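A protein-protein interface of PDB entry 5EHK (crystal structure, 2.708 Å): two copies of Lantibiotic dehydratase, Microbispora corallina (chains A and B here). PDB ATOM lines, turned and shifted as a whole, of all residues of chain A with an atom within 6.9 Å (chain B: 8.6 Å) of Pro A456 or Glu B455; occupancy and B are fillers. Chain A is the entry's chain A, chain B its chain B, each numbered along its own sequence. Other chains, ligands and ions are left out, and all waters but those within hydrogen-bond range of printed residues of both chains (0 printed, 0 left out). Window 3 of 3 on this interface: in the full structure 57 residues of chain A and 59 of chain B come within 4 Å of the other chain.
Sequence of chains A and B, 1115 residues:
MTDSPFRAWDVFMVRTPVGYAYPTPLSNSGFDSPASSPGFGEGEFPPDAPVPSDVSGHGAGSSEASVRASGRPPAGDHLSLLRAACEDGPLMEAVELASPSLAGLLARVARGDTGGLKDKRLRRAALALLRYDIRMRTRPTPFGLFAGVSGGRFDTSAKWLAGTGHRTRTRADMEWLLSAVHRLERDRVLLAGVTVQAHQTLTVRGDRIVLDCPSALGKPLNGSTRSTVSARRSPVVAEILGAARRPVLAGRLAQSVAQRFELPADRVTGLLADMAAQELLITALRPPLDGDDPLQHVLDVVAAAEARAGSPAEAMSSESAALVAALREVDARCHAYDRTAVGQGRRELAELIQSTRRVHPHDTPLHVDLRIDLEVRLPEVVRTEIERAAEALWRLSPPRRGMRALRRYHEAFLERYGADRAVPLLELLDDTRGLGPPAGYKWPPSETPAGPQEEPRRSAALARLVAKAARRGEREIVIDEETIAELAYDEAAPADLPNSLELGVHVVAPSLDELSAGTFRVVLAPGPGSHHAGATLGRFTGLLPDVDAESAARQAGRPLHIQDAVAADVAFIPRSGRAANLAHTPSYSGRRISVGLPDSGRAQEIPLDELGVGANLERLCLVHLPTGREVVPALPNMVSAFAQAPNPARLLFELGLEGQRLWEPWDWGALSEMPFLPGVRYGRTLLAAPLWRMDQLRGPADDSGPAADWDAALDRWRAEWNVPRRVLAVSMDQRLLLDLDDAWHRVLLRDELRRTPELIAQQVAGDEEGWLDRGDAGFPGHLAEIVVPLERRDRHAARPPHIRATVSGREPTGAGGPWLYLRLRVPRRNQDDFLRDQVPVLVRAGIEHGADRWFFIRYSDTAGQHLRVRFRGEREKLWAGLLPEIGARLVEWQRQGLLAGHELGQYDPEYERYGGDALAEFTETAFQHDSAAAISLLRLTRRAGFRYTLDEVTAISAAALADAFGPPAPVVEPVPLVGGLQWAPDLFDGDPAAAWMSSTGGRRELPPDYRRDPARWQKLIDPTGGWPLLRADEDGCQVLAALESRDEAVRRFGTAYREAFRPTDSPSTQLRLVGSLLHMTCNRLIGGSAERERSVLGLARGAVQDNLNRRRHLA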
ATOM      1  N   GLN A 453     -26.649  15.340  14.334  1.00  0.00           N
ATOM      2  CA  GLN A 453     -25.214  15.129  14.530  1.00  0.00           C
ATOM      3  C   GLN A 453     -25.007  13.841  15.346  1.00  0.00           C
ATOM      4  O   GLN A 453     -25.936  13.358  15.996  1.00  0.00           O
ATOM      5  CB  GLN A 453     -24.602  16.335  15.257  1.00  0.00           C
ATOM      6  CG  GLN A 453     -23.082  16.294  15.443  1.00  0.00           C
ATOM      7  CD  GLN A 453     -22.303  16.420  14.140  1.00  0.00           C
ATOM      8  OE1 GLN A 453     -22.046  15.427  13.453  1.00  0.00           O
ATOM      9  NE2 GLN A 453     -21.872  17.639  13.827  1.00  0.00           N
ATOM     10  N   GLU A 454     -23.836  13.224  15.248  1.00  0.00           N
ATOM     11  CA  GLU A 454     -23.601  12.012  16.026  1.00  0.00           C
ATOM     12  C   GLU A 454     -23.002  12.384  17.396  1.00  0.00           C
ATOM     13  O   GLU A 454     -22.008  13.118  17.474  1.00  0.00           O
ATOM     14  CB  GLU A 454     -22.711  11.035  15.251  1.00  0.00           C
ATOM     15  CG  GLU A 454     -23.033   9.564  15.519  1.00  0.00           C
ATOM     16  CD  GLU A 454     -22.150   8.592  14.718  1.00  0.00           C
ATOM     17  OE1 GLU A 454     -21.140   9.020  14.106  1.00  0.00           O
ATOM     18  OE2 GLU A 454     -22.475   7.387  14.701  1.00  0.00           O
ATOM     19  N   GLU A 455     -23.627  11.900  18.470  1.00  0.00           N
ATOM     20  CA  GLU A 455     -23.102  12.097  19.830  1.00  0.00           C
ATOM     21  C   GLU A 455     -21.799  11.321  20.026  1.00  0.00           C
ATOM     22  O   GLU A 455     -21.699  10.166  19.620  1.00  0.00           O
ATOM     23  CB  GLU A 455     -24.121  11.623  20.874  1.00  0.00           C
ATOM     24  CG  GLU A 455     -25.178  12.653  21.269  1.00  0.00           C
ATOM     25  CD  GLU A 455     -26.059  12.174  22.428  1.00  0.00           C
ATOM     26  OE1 GLU A 455     -27.152  12.754  22.645  1.00  0.00           O
ATOM     27  OE2 GLU A 455     -25.664  11.203  23.115  1.00  0.00           O
ATOM     28  N   PRO A 456     -20.795  11.945  20.654  1.00  0.00           N
ATOM     29  CA  PRO A 456     -19.621  11.176  21.073  1.00  0.00           C
ATOM     30  C   PRO A 456     -20.103  10.017  21.923  1.00  0.00           C
ATOM     31  O   PRO A 456     -21.052  10.180  22.698  1.00  0.00           O
ATOM     32  CB  PRO A 456     -18.826  12.170  21.915  1.00  0.00           C
ATOM     33  CG  PRO A 456     -19.235  13.500  21.422  1.00  0.00           C
ATOM     34  CD  PRO A 456     -20.677  13.371  21.002  1.00  0.00           C
ATOM     35  N   ARG A 457     -19.502   8.848  21.739  1.00  0.00           N
ATOM     36  CA  ARG A 457     -20.023   7.631  22.349  1.00  0.00           C
ATOM     37  C   ARG A 457     -19.985   7.696  23.873  1.00  0.00           C
ATOM     38  O   ARG A 457     -19.174   8.414  24.458  1.00  0.00           O
ATOM     39  CB  ARG A 457     -19.222   6.424  21.866  1.00  0.00           C
ATOM     40  CG  ARG A 457     -19.774   5.100  22.335  1.00  0.00           C
ATOM     41  CD  ARG A 457     -18.807   4.009  22.069  1.00  0.00           C
ATOM     42  NE  ARG A 457     -19.402   2.707  22.333  1.00  0.00           N
ATOM     43  CZ  ARG A 457     -18.784   1.567  22.071  1.00  0.00           C
ATOM     44  NH1 ARG A 457     -17.567   1.603  21.532  1.00  0.00           N
ATOM     45  NH2 ARG A 457     -19.361   0.405  22.342  1.00  0.00           N
ATOM     46  N   ARG A 458     -20.891   6.970  24.509  1.00  0.00           N
ATOM     47  CA  ARG A 458     -20.877   6.848  25.959  1.00  0.00           C
ATOM     48  C   ARG A 458     -20.998   5.393  26.356  1.00  0.00           C
ATOM     49  O   ARG A 458     -21.927   4.705  25.934  1.00  0.00           O
ATOM     50  CB  ARG A 458     -21.983   7.708  26.607  1.00  0.00           C
ATOM     51  CG  ARG A 458     -21.973   9.180  26.154  1.00  0.00           C
ATOM     52  CD  ARG A 458     -23.053  10.014  26.817  1.00  0.00           C
ATOM     53  NE  ARG A 458     -24.123  10.328  25.868  1.00  0.00           N
ATOM     54  CZ  ARG A 458     -25.313   9.735  25.877  1.00  0.00           C
ATOM     55  NH1 ARG A 458     -25.594   8.817  26.794  1.00  0.00           N
ATOM     56  NH2 ARG A 458     -26.225  10.069  24.983  1.00  0.00           N
ATOM     57  N   ASP A 667     -12.341   4.328  19.279  1.00  0.00           N
ATOM     58  CA  ASP A 667     -13.200   5.460  19.624  1.00  0.00           C
ATOM     59  C   ASP A 667     -13.430   5.606  21.150  1.00  0.00           C
ATOM     60  O   ASP A 667     -14.071   4.762  21.799  1.00  0.00           O
ATOM     61  CB  ASP A 667     -14.520   5.360  18.843  1.00  0.00           C
ATOM     62  CG  ASP A 667     -15.427   6.557  19.063  1.00  0.00           C
ATOM     63  OD1 ASP A 667     -14.909   7.669  19.270  1.00  0.00           O
ATOM     64  OD2 ASP A 667     -16.658   6.394  18.976  1.00  0.00           O
ATOM     65  N   TRP A 668     -12.884   6.689  21.704  1.00  0.00           N
ATOM     66  CA  TRP A 668     -12.951   6.957  23.137  1.00  0.00           C
ATOM     67  C   TRP A 668     -14.269   7.624  23.500  1.00  0.00           C
ATOM     68  O   TRP A 668     -14.664   7.636  24.669  1.00  0.00           O
ATOM     69  CB  TRP A 668     -11.786   7.826  23.603  1.00  0.00           C
ATOM     70  CG  TRP A 668     -10.556   7.066  24.092  1.00  0.00           C
ATOM     71  CD1 TRP A 668      -9.276   7.181  23.618  1.00  0.00           C
ATOM     72  CD2 TRP A 668     -10.501   6.101  25.157  1.00  0.00           C
ATOM     73  NE1 TRP A 668      -8.434   6.356  24.323  1.00  0.00           N
ATOM     74  CE2 TRP A 668      -9.159   5.676  25.268  1.00  0.00           C
ATOM     75  CE3 TRP A 668     -11.452   5.556  26.021  1.00  0.00           C
ATOM     76  CZ2 TRP A 668      -8.746   4.732  26.214  1.00  0.00           C
ATOM     77  CZ3 TRP A 668     -11.041   4.616  26.954  1.00  0.00           C
ATOM     78  CH2 TRP A 668      -9.697   4.217  27.045  1.00  0.00           C
ATOM     79  N   GLY A 669     -14.936   8.194  22.497  1.00  0.00           N
ATOM     80  CA  GLY A 669     -16.233   8.803  22.712  1.00  0.00           C
ATOM     81  C   GLY A 669     -16.157   9.998  23.639  1.00  0.00           C
ATOM     82  O   GLY A 669     -15.218  10.790  23.560  1.00  0.00           O
ATOM     83  N   ALA A 670     -17.156  10.128  24.506  1.00  0.00           N
ATOM     84  CA  ALA A 670     -17.228  11.231  25.464  1.00  0.00           C
ATOM     85  C   ALA A 670     -15.984  11.272  26.347  1.00  0.00           C
ATOM     86  O   ALA A 670     -15.548  12.359  26.783  1.00  0.00           O
ATOM     87  CB  ALA A 670     -18.457  11.093  26.330  1.00  0.00           C
ATOM     88  N   LEU A 671     -15.398  10.090  26.570  1.00  0.00           N
ATOM     89  CA  LEU A 671     -14.265   9.942  27.468  1.00  0.00           C
ATOM     90  C   LEU A 671     -13.050  10.684  26.978  1.00  0.00           C
ATOM     91  O   LEU A 671     -12.067  10.797  27.683  1.00  0.00           O
ATOM     92  CB  LEU A 671     -13.933   8.476  27.716  1.00  0.00           C
ATOM     93  CG  LEU A 671     -14.817   7.841  28.785  1.00  0.00           C
ATOM     94  CD1 LEU A 671     -14.728   6.329  28.784  1.00  0.00           C
ATOM     95  CD2 LEU A 671     -14.441   8.410  30.159  1.00  0.00           C
ATOM     96  N   SER A 672     -13.144  11.260  25.796  1.00  0.00           N
ATOM     97  CA  SER A 672     -12.027  11.990  25.225  1.00  0.00           C
ATOM     98  C   SER A 672     -11.700  13.255  26.025  1.00  0.00           C
ATOM     99  O   SER A 672     -10.643  13.873  25.836  1.00  0.00           O
ATOM    100  CB  SER A 672     -12.325  12.298  23.756  1.00  0.00           C
ATOM    101  OG  SER A 672     -11.954  13.609  23.418  1.00  0.00           O
ATOM    102  N   GLU A 673     -12.595  13.620  26.940  1.00  0.00           N
ATOM    103  CA  GLU A 673     -12.413  14.832  27.737  1.00  0.00           C
ATOM    104  C   GLU A 673     -11.469  14.634  28.935  1.00  0.00           C
ATOM    105  O   GLU A 673     -10.953  15.620  29.484  1.00  0.00           O
ATOM    106  CB  GLU A 673     -13.758  15.359  28.237  1.00  0.00           C
ATOM    107  CG  GLU A 673     -14.750  15.712  27.134  1.00  0.00           C
ATOM    108  CD  GLU A 673     -14.222  16.789  26.192  1.00  0.00           C
ATOM    109  OE1 GLU A 673     -13.594  17.758  26.682  1.00  0.00           O
ATOM    110  OE2 GLU A 673     -14.448  16.666  24.962  1.00  0.00           O
ATOM    111  N   ARG B 404     -36.523  25.743  28.379  1.00  0.00           N
ATOM    112  CA  ARG B 404     -36.030  25.330  27.071  1.00  0.00           C
ATOM    113  C   ARG B 404     -37.176  24.993  26.097  1.00  0.00           C
ATOM    114  O   ARG B 404     -37.095  25.309  24.903  1.00  0.00           O
ATOM    115  CB  ARG B 404     -35.060  24.167  27.213  1.00  0.00           C
ATOM    116  CG  ARG B 404     -34.269  23.907  25.974  1.00  0.00           C
ATOM    117  CD  ARG B 404     -33.316  22.736  26.178  1.00  0.00           C
ATOM    118  NE  ARG B 404     -32.546  22.428  24.967  1.00  0.00           N
ATOM    119  CZ  ARG B 404     -32.879  21.507  24.070  1.00  0.00           C
ATOM    120  NH1 ARG B 404     -33.970  20.762  24.242  1.00  0.00           N
ATOM    121  NH2 ARG B 404     -32.098  21.319  23.010  1.00  0.00           N
ATOM    122  N   PRO B 452     -33.186  19.984  17.454  1.00  0.00           N
ATOM    123  CA  PRO B 452     -32.029  19.129  17.739  1.00  0.00           C
ATOM    124  C   PRO B 452     -31.990  18.735  19.213  1.00  0.00           C
ATOM    125  O   PRO B 452     -32.170  19.594  20.096  1.00  0.00           O
ATOM    126  CB  PRO B 452     -30.831  20.043  17.423  1.00  0.00           C
ATOM    127  CG  PRO B 452     -31.336  21.037  16.445  1.00  0.00           C
ATOM    128  CD  PRO B 452     -32.785  21.264  16.837  1.00  0.00           C
ATOM    129  N   GLN B 453     -31.772  17.451  19.481  1.00  0.00           N
ATOM    130  CA  GLN B 453     -31.647  17.005  20.863  1.00  0.00           C
ATOM    131  C   GLN B 453     -30.382  17.582  21.516  1.00  0.00           C
ATOM    132  O   GLN B 453     -29.381  17.848  20.843  1.00  0.00           O
ATOM    133  CB  GLN B 453     -31.702  15.480  20.950  1.00  0.00           C
ATOM    134  CG  GLN B 453     -31.635  14.924  22.368  1.00  0.00           C
ATOM    135  CD  GLN B 453     -32.832  15.324  23.225  1.00  0.00           C
ATOM    136  OE1 GLN B 453     -32.820  16.367  23.901  1.00  0.00           O
ATOM    137  NE2 GLN B 453     -33.875  14.498  23.199  1.00  0.00           N
ATOM    138  N   GLU B 454     -30.427  17.758  22.833  1.00  0.00           N
ATOM    139  CA  GLU B 454     -29.326  18.367  23.568  1.00  0.00           C
ATOM    140  C   GLU B 454     -28.338  17.277  23.969  1.00  0.00           C
ATOM    141  O   GLU B 454     -28.730  16.265  24.570  1.00  0.00           O
ATOM    142  CB  GLU B 454     -29.875  19.062  24.818  1.00  0.00           C
ATOM    143  CG  GLU B 454     -29.138  20.320  25.249  1.00  0.00           C
ATOM    144  CD  GLU B 454     -29.758  20.965  26.497  1.00  0.00           C
ATOM    145  OE1 GLU B 454     -30.602  20.313  27.160  1.00  0.00           O
ATOM    146  OE2 GLU B 454     -29.424  22.134  26.802  1.00  0.00           O
ATOM    147  N   GLU B 455     -27.066  17.470  23.618  1.00  0.00           N
ATOM    148  CA  GLU B 455     -26.007  16.554  24.051  1.00  0.00           C
ATOM    149  C   GLU B 455     -25.762  16.625  25.566  1.00  0.00           C
ATOM    150  O   GLU B 455     -25.690  17.726  26.129  1.00  0.00           O
ATOM    151  CB  GLU B 455     -24.684  16.874  23.349  1.00  0.00           C
ATOM    152  CG  GLU B 455     -24.472  16.207  22.001  1.00  0.00           C
ATOM    153  CD  GLU B 455     -23.036  16.384  21.494  1.00  0.00           C
ATOM    154  OE1 GLU B 455     -22.784  16.136  20.287  1.00  0.00           O
ATOM    155  OE2 GLU B 455     -22.156  16.754  22.316  1.00  0.00           O
ATOM    156  N   PRO B 456     -25.622  15.453  26.223  1.00  0.00           N
ATOM    157  CA  PRO B 456     -25.109  15.453  27.600  1.00  0.00           C
ATOM    158  C   PRO B 456     -23.795  16.204  27.607  1.00  0.00           C
ATOM    159  O   PRO B 456     -22.976  16.024  26.713  1.00  0.00           O
ATOM    160  CB  PRO B 456     -24.883  13.969  27.893  1.00  0.00           C
ATOM    161  CG  PRO B 456     -25.882  13.263  26.994  1.00  0.00           C
ATOM    162  CD  PRO B 456     -26.008  14.107  25.760  1.00  0.00           C
ATOM    163  N   ARG B 457     -23.607  17.063  28.598  1.00  0.00           N
ATOM    164  CA  ARG B 457     -22.490  17.989  28.569  1.00  0.00           C
ATOM    165  C   ARG B 457     -21.172  17.250  28.631  1.00  0.00           C
ATOM    166  O   ARG B 457     -21.081  16.169  29.225  1.00  0.00           O
ATOM    167  CB  ARG B 457     -22.598  18.958  29.737  1.00  0.00           C
ATOM    168  CG  ARG B 457     -21.550  20.045  29.761  1.00  0.00           C
ATOM    169  CD  ARG B 457     -21.587  20.721  31.103  1.00  0.00           C
ATOM    170  NE  ARG B 457     -20.718  21.887  31.161  1.00  0.00           N
ATOM    171  CZ  ARG B 457     -20.652  22.694  32.211  1.00  0.00           C
ATOM    172  NH1 ARG B 457     -21.414  22.446  33.278  1.00  0.00           N
ATOM    173  NH2 ARG B 457     -19.829  23.738  32.192  1.00  0.00           N
ATOM    174  N   ARG B 458     -20.154  17.854  28.026  1.00  0.00           N
ATOM    175  CA  ARG B 458     -18.797  17.333  28.082  1.00  0.00           C
ATOM    176  C   ARG B 458     -17.881  18.474  28.495  1.00  0.00           C
ATOM    177  O   ARG B 458     -17.965  19.568  27.959  1.00  0.00           O
ATOM    178  CB  ARG B 458     -18.369  16.770  26.725  1.00  0.00           C
ATOM    179  CG  ARG B 458     -19.371  15.814  26.078  1.00  0.00           C
ATOM    180  CD  ARG B 458     -18.826  15.273  24.768  1.00  0.00           C
ATOM    181  NE  ARG B 458     -19.478  15.888  23.615  1.00  0.00           N
ATOM    182  CZ  ARG B 458     -18.910  16.818  22.851  1.00  0.00           C
ATOM    183  NH1 ARG B 458     -17.674  17.235  23.109  1.00  0.00           N
ATOM    184  NH2 ARG B 458     -19.576  17.327  21.825  1.00  0.00           N
ATOM    185  N   TYR B 489     -20.858  28.610  32.177  1.00  0.00           N
ATOM    186  CA  TYR B 489     -20.985  28.844  30.747  1.00  0.00           C
ATOM    187  C   TYR B 489     -20.801  30.325  30.428  1.00  0.00           C
ATOM    188  O   TYR B 489     -20.466  30.678  29.302  1.00  0.00           O
ATOM    189  CB  TYR B 489     -22.341  28.402  30.234  1.00  0.00           C
ATOM    190  CG  TYR B 489     -22.656  26.914  30.325  1.00  0.00           C
ATOM    191  CD1 TYR B 489     -22.217  26.008  29.345  1.00  0.00           C
ATOM    192  CD2 TYR B 489     -23.465  26.433  31.346  1.00  0.00           C
ATOM    193  CE1 TYR B 489     -22.545  24.669  29.414  1.00  0.00           C
ATOM    194  CE2 TYR B 489     -23.806  25.086  31.422  1.00  0.00           C
ATOM    195  CZ  TYR B 489     -23.348  24.208  30.459  1.00  0.00           C
ATOM    196  OH  TYR B 489     -23.717  22.881  30.564  1.00  0.00           O
ATOM    197  N   ASP B 667     -25.185  19.152  37.068  1.00  0.00           N
ATOM    198  CA  ASP B 667     -25.241  18.317  35.868  1.00  0.00           C
ATOM    199  C   ASP B 667     -23.894  17.689  35.496  1.00  0.00           C
ATOM    200  O   ASP B 667     -22.953  18.400  35.108  1.00  0.00           O
ATOM    201  CB  ASP B 667     -25.756  19.104  34.676  1.00  0.00           C
ATOM    202  CG  ASP B 667     -25.928  18.241  33.438  1.00  0.00           C
ATOM    203  OD1 ASP B 667     -26.306  17.057  33.567  1.00  0.00           O
ATOM    204  OD2 ASP B 667     -25.663  18.748  32.331  1.00  0.00           O
ATOM    205  N   GLY B 669     -23.482  15.506  33.105  1.00  0.00           N
ATOM    206  CA  GLY B 669     -23.426  15.347  31.662  1.00  0.00           C
ATOM    207  C   GLY B 669     -22.938  13.971  31.246  1.00  0.00           C
ATOM    208  O   GLY B 669     -23.268  12.965  31.875  1.00  0.00           O
ATOM    209  N   ALA B 670     -22.122  13.932  30.199  1.00  0.00           N
ATOM    210  CA  ALA B 670     -21.615  12.667  29.646  1.00  0.00           C
ATOM    211  C   ALA B 670     -20.891  11.779  30.668  1.00  0.00           C
ATOM    212  O   ALA B 670     -20.881  10.542  30.534  1.00  0.00           O
ATOM    213  CB  ALA B 670     -20.726  12.935  28.442  1.00  0.00           C
ATOM    214  N   GLU B 673     -21.452   8.129  32.975  1.00  0.00           N
ATOM    215  CA  GLU B 673     -21.159   6.726  32.693  1.00  0.00           C
ATOM    216  C   GLU B 673     -20.082   6.173  33.625  1.00  0.00           C
ATOM    217  O   GLU B 673     -19.955   4.953  33.765  1.00  0.00           O
ATOM    218  CB  GLU B 673     -20.715   6.534  31.234  1.00  0.00           C
ATOM    219  CG  GLU B 673     -21.733   6.963  30.190  1.00  0.00           C
ATOM    220  CD  GLU B 673     -23.037   6.202  30.319  1.00  0.00           C
ATOM    221  OE1 GLU B 673     -22.994   4.977  30.560  1.00  0.00           O
ATOM    222  OE2 GLU B 673     -24.109   6.829  30.173  1.00  0.00           O
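OE2 of Glu A673 is in salt-bridge range of NH1 of Arg B458.
The guanidinium group (NE) of Arg A458 is in salt-bridge range of the side-chain carboxylate (OE2) of Glu A455 (3.3 Å).
N of Ala A670 lies within hydrogen-bond range of O of Arg A457 (2.6 Å).
NH2 of Arg B458 is in salt-bridge range of OE2 of Glu B455.
The backbone NH (N) of Ala B670 is in hydrogen-bond range of the backbone carbonyl oxygen (O) of Arg B457, 2.7 Å away.
Among the printed residues, merely in contact across the chains: Pro A456 with Arg B458, Pro A456 with Glu B455, Glu A455 with Pro B456, Arg A458 with Pro B456, Ala A670 with Ala B670, Arg A458 with Glu B673 and Glu A455 with Glu B455.
Printed residues of chain B within 4 Å of Pro A456: Glu B455 (3.5 Å) and Arg B458 (3.3 Å).
Of chain A, only Glu A455 and Pro A456 come within 4 Å of Glu B455.
Printed residues of chain B within 4 Å of Glu A455: Glu B455 (3.7 Å) and Pro B456 (3.6 Å).
Of the printed residues of chain B, Glu A673 touches Arg B458.
Of the printed residues of chain A, Glu B673 touches Arg A458.
Printed residues of chain B within 4 Å of Arg A458: Pro B456 and Glu B673.
Of the printed residues of chain A, Arg B458 touches Pro A456 and Glu A673.
Arg A457 touches none of the printed residues of chain B.
Gln A453 touches none of the printed residues of chain B.
The nearest residue of chain A that does not touch Glu B455 is Glu A454 (4.2 Å).
Printed residues of chain A that touch a printed residue of chain B: Glu A455, Pro A456, Arg A458, Ala A670 and Glu A673.
Hydrophobic or aromatic side chains of chain A within 4 Å of the printed part of chain B: Pro A456 and Ala A670.
Of the 13 printed residues of chain B, 5 touch a printed residue of chain A.
Along chain B the printed residues that touch a printed residue of chain A span positions 455 to 673.
Glu A455 touches Pro B456, and with the chains exchanged Pro A456 touches Glu B455.
Pro A456 touches Arg B458, and with the chains exchanged Arg A458 touches Pro B456.
Arg A458 touches Glu B673, and with the chains exchanged Glu A673 touches Arg B458.
Ala B670 touches its own counterpart, Ala A670.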
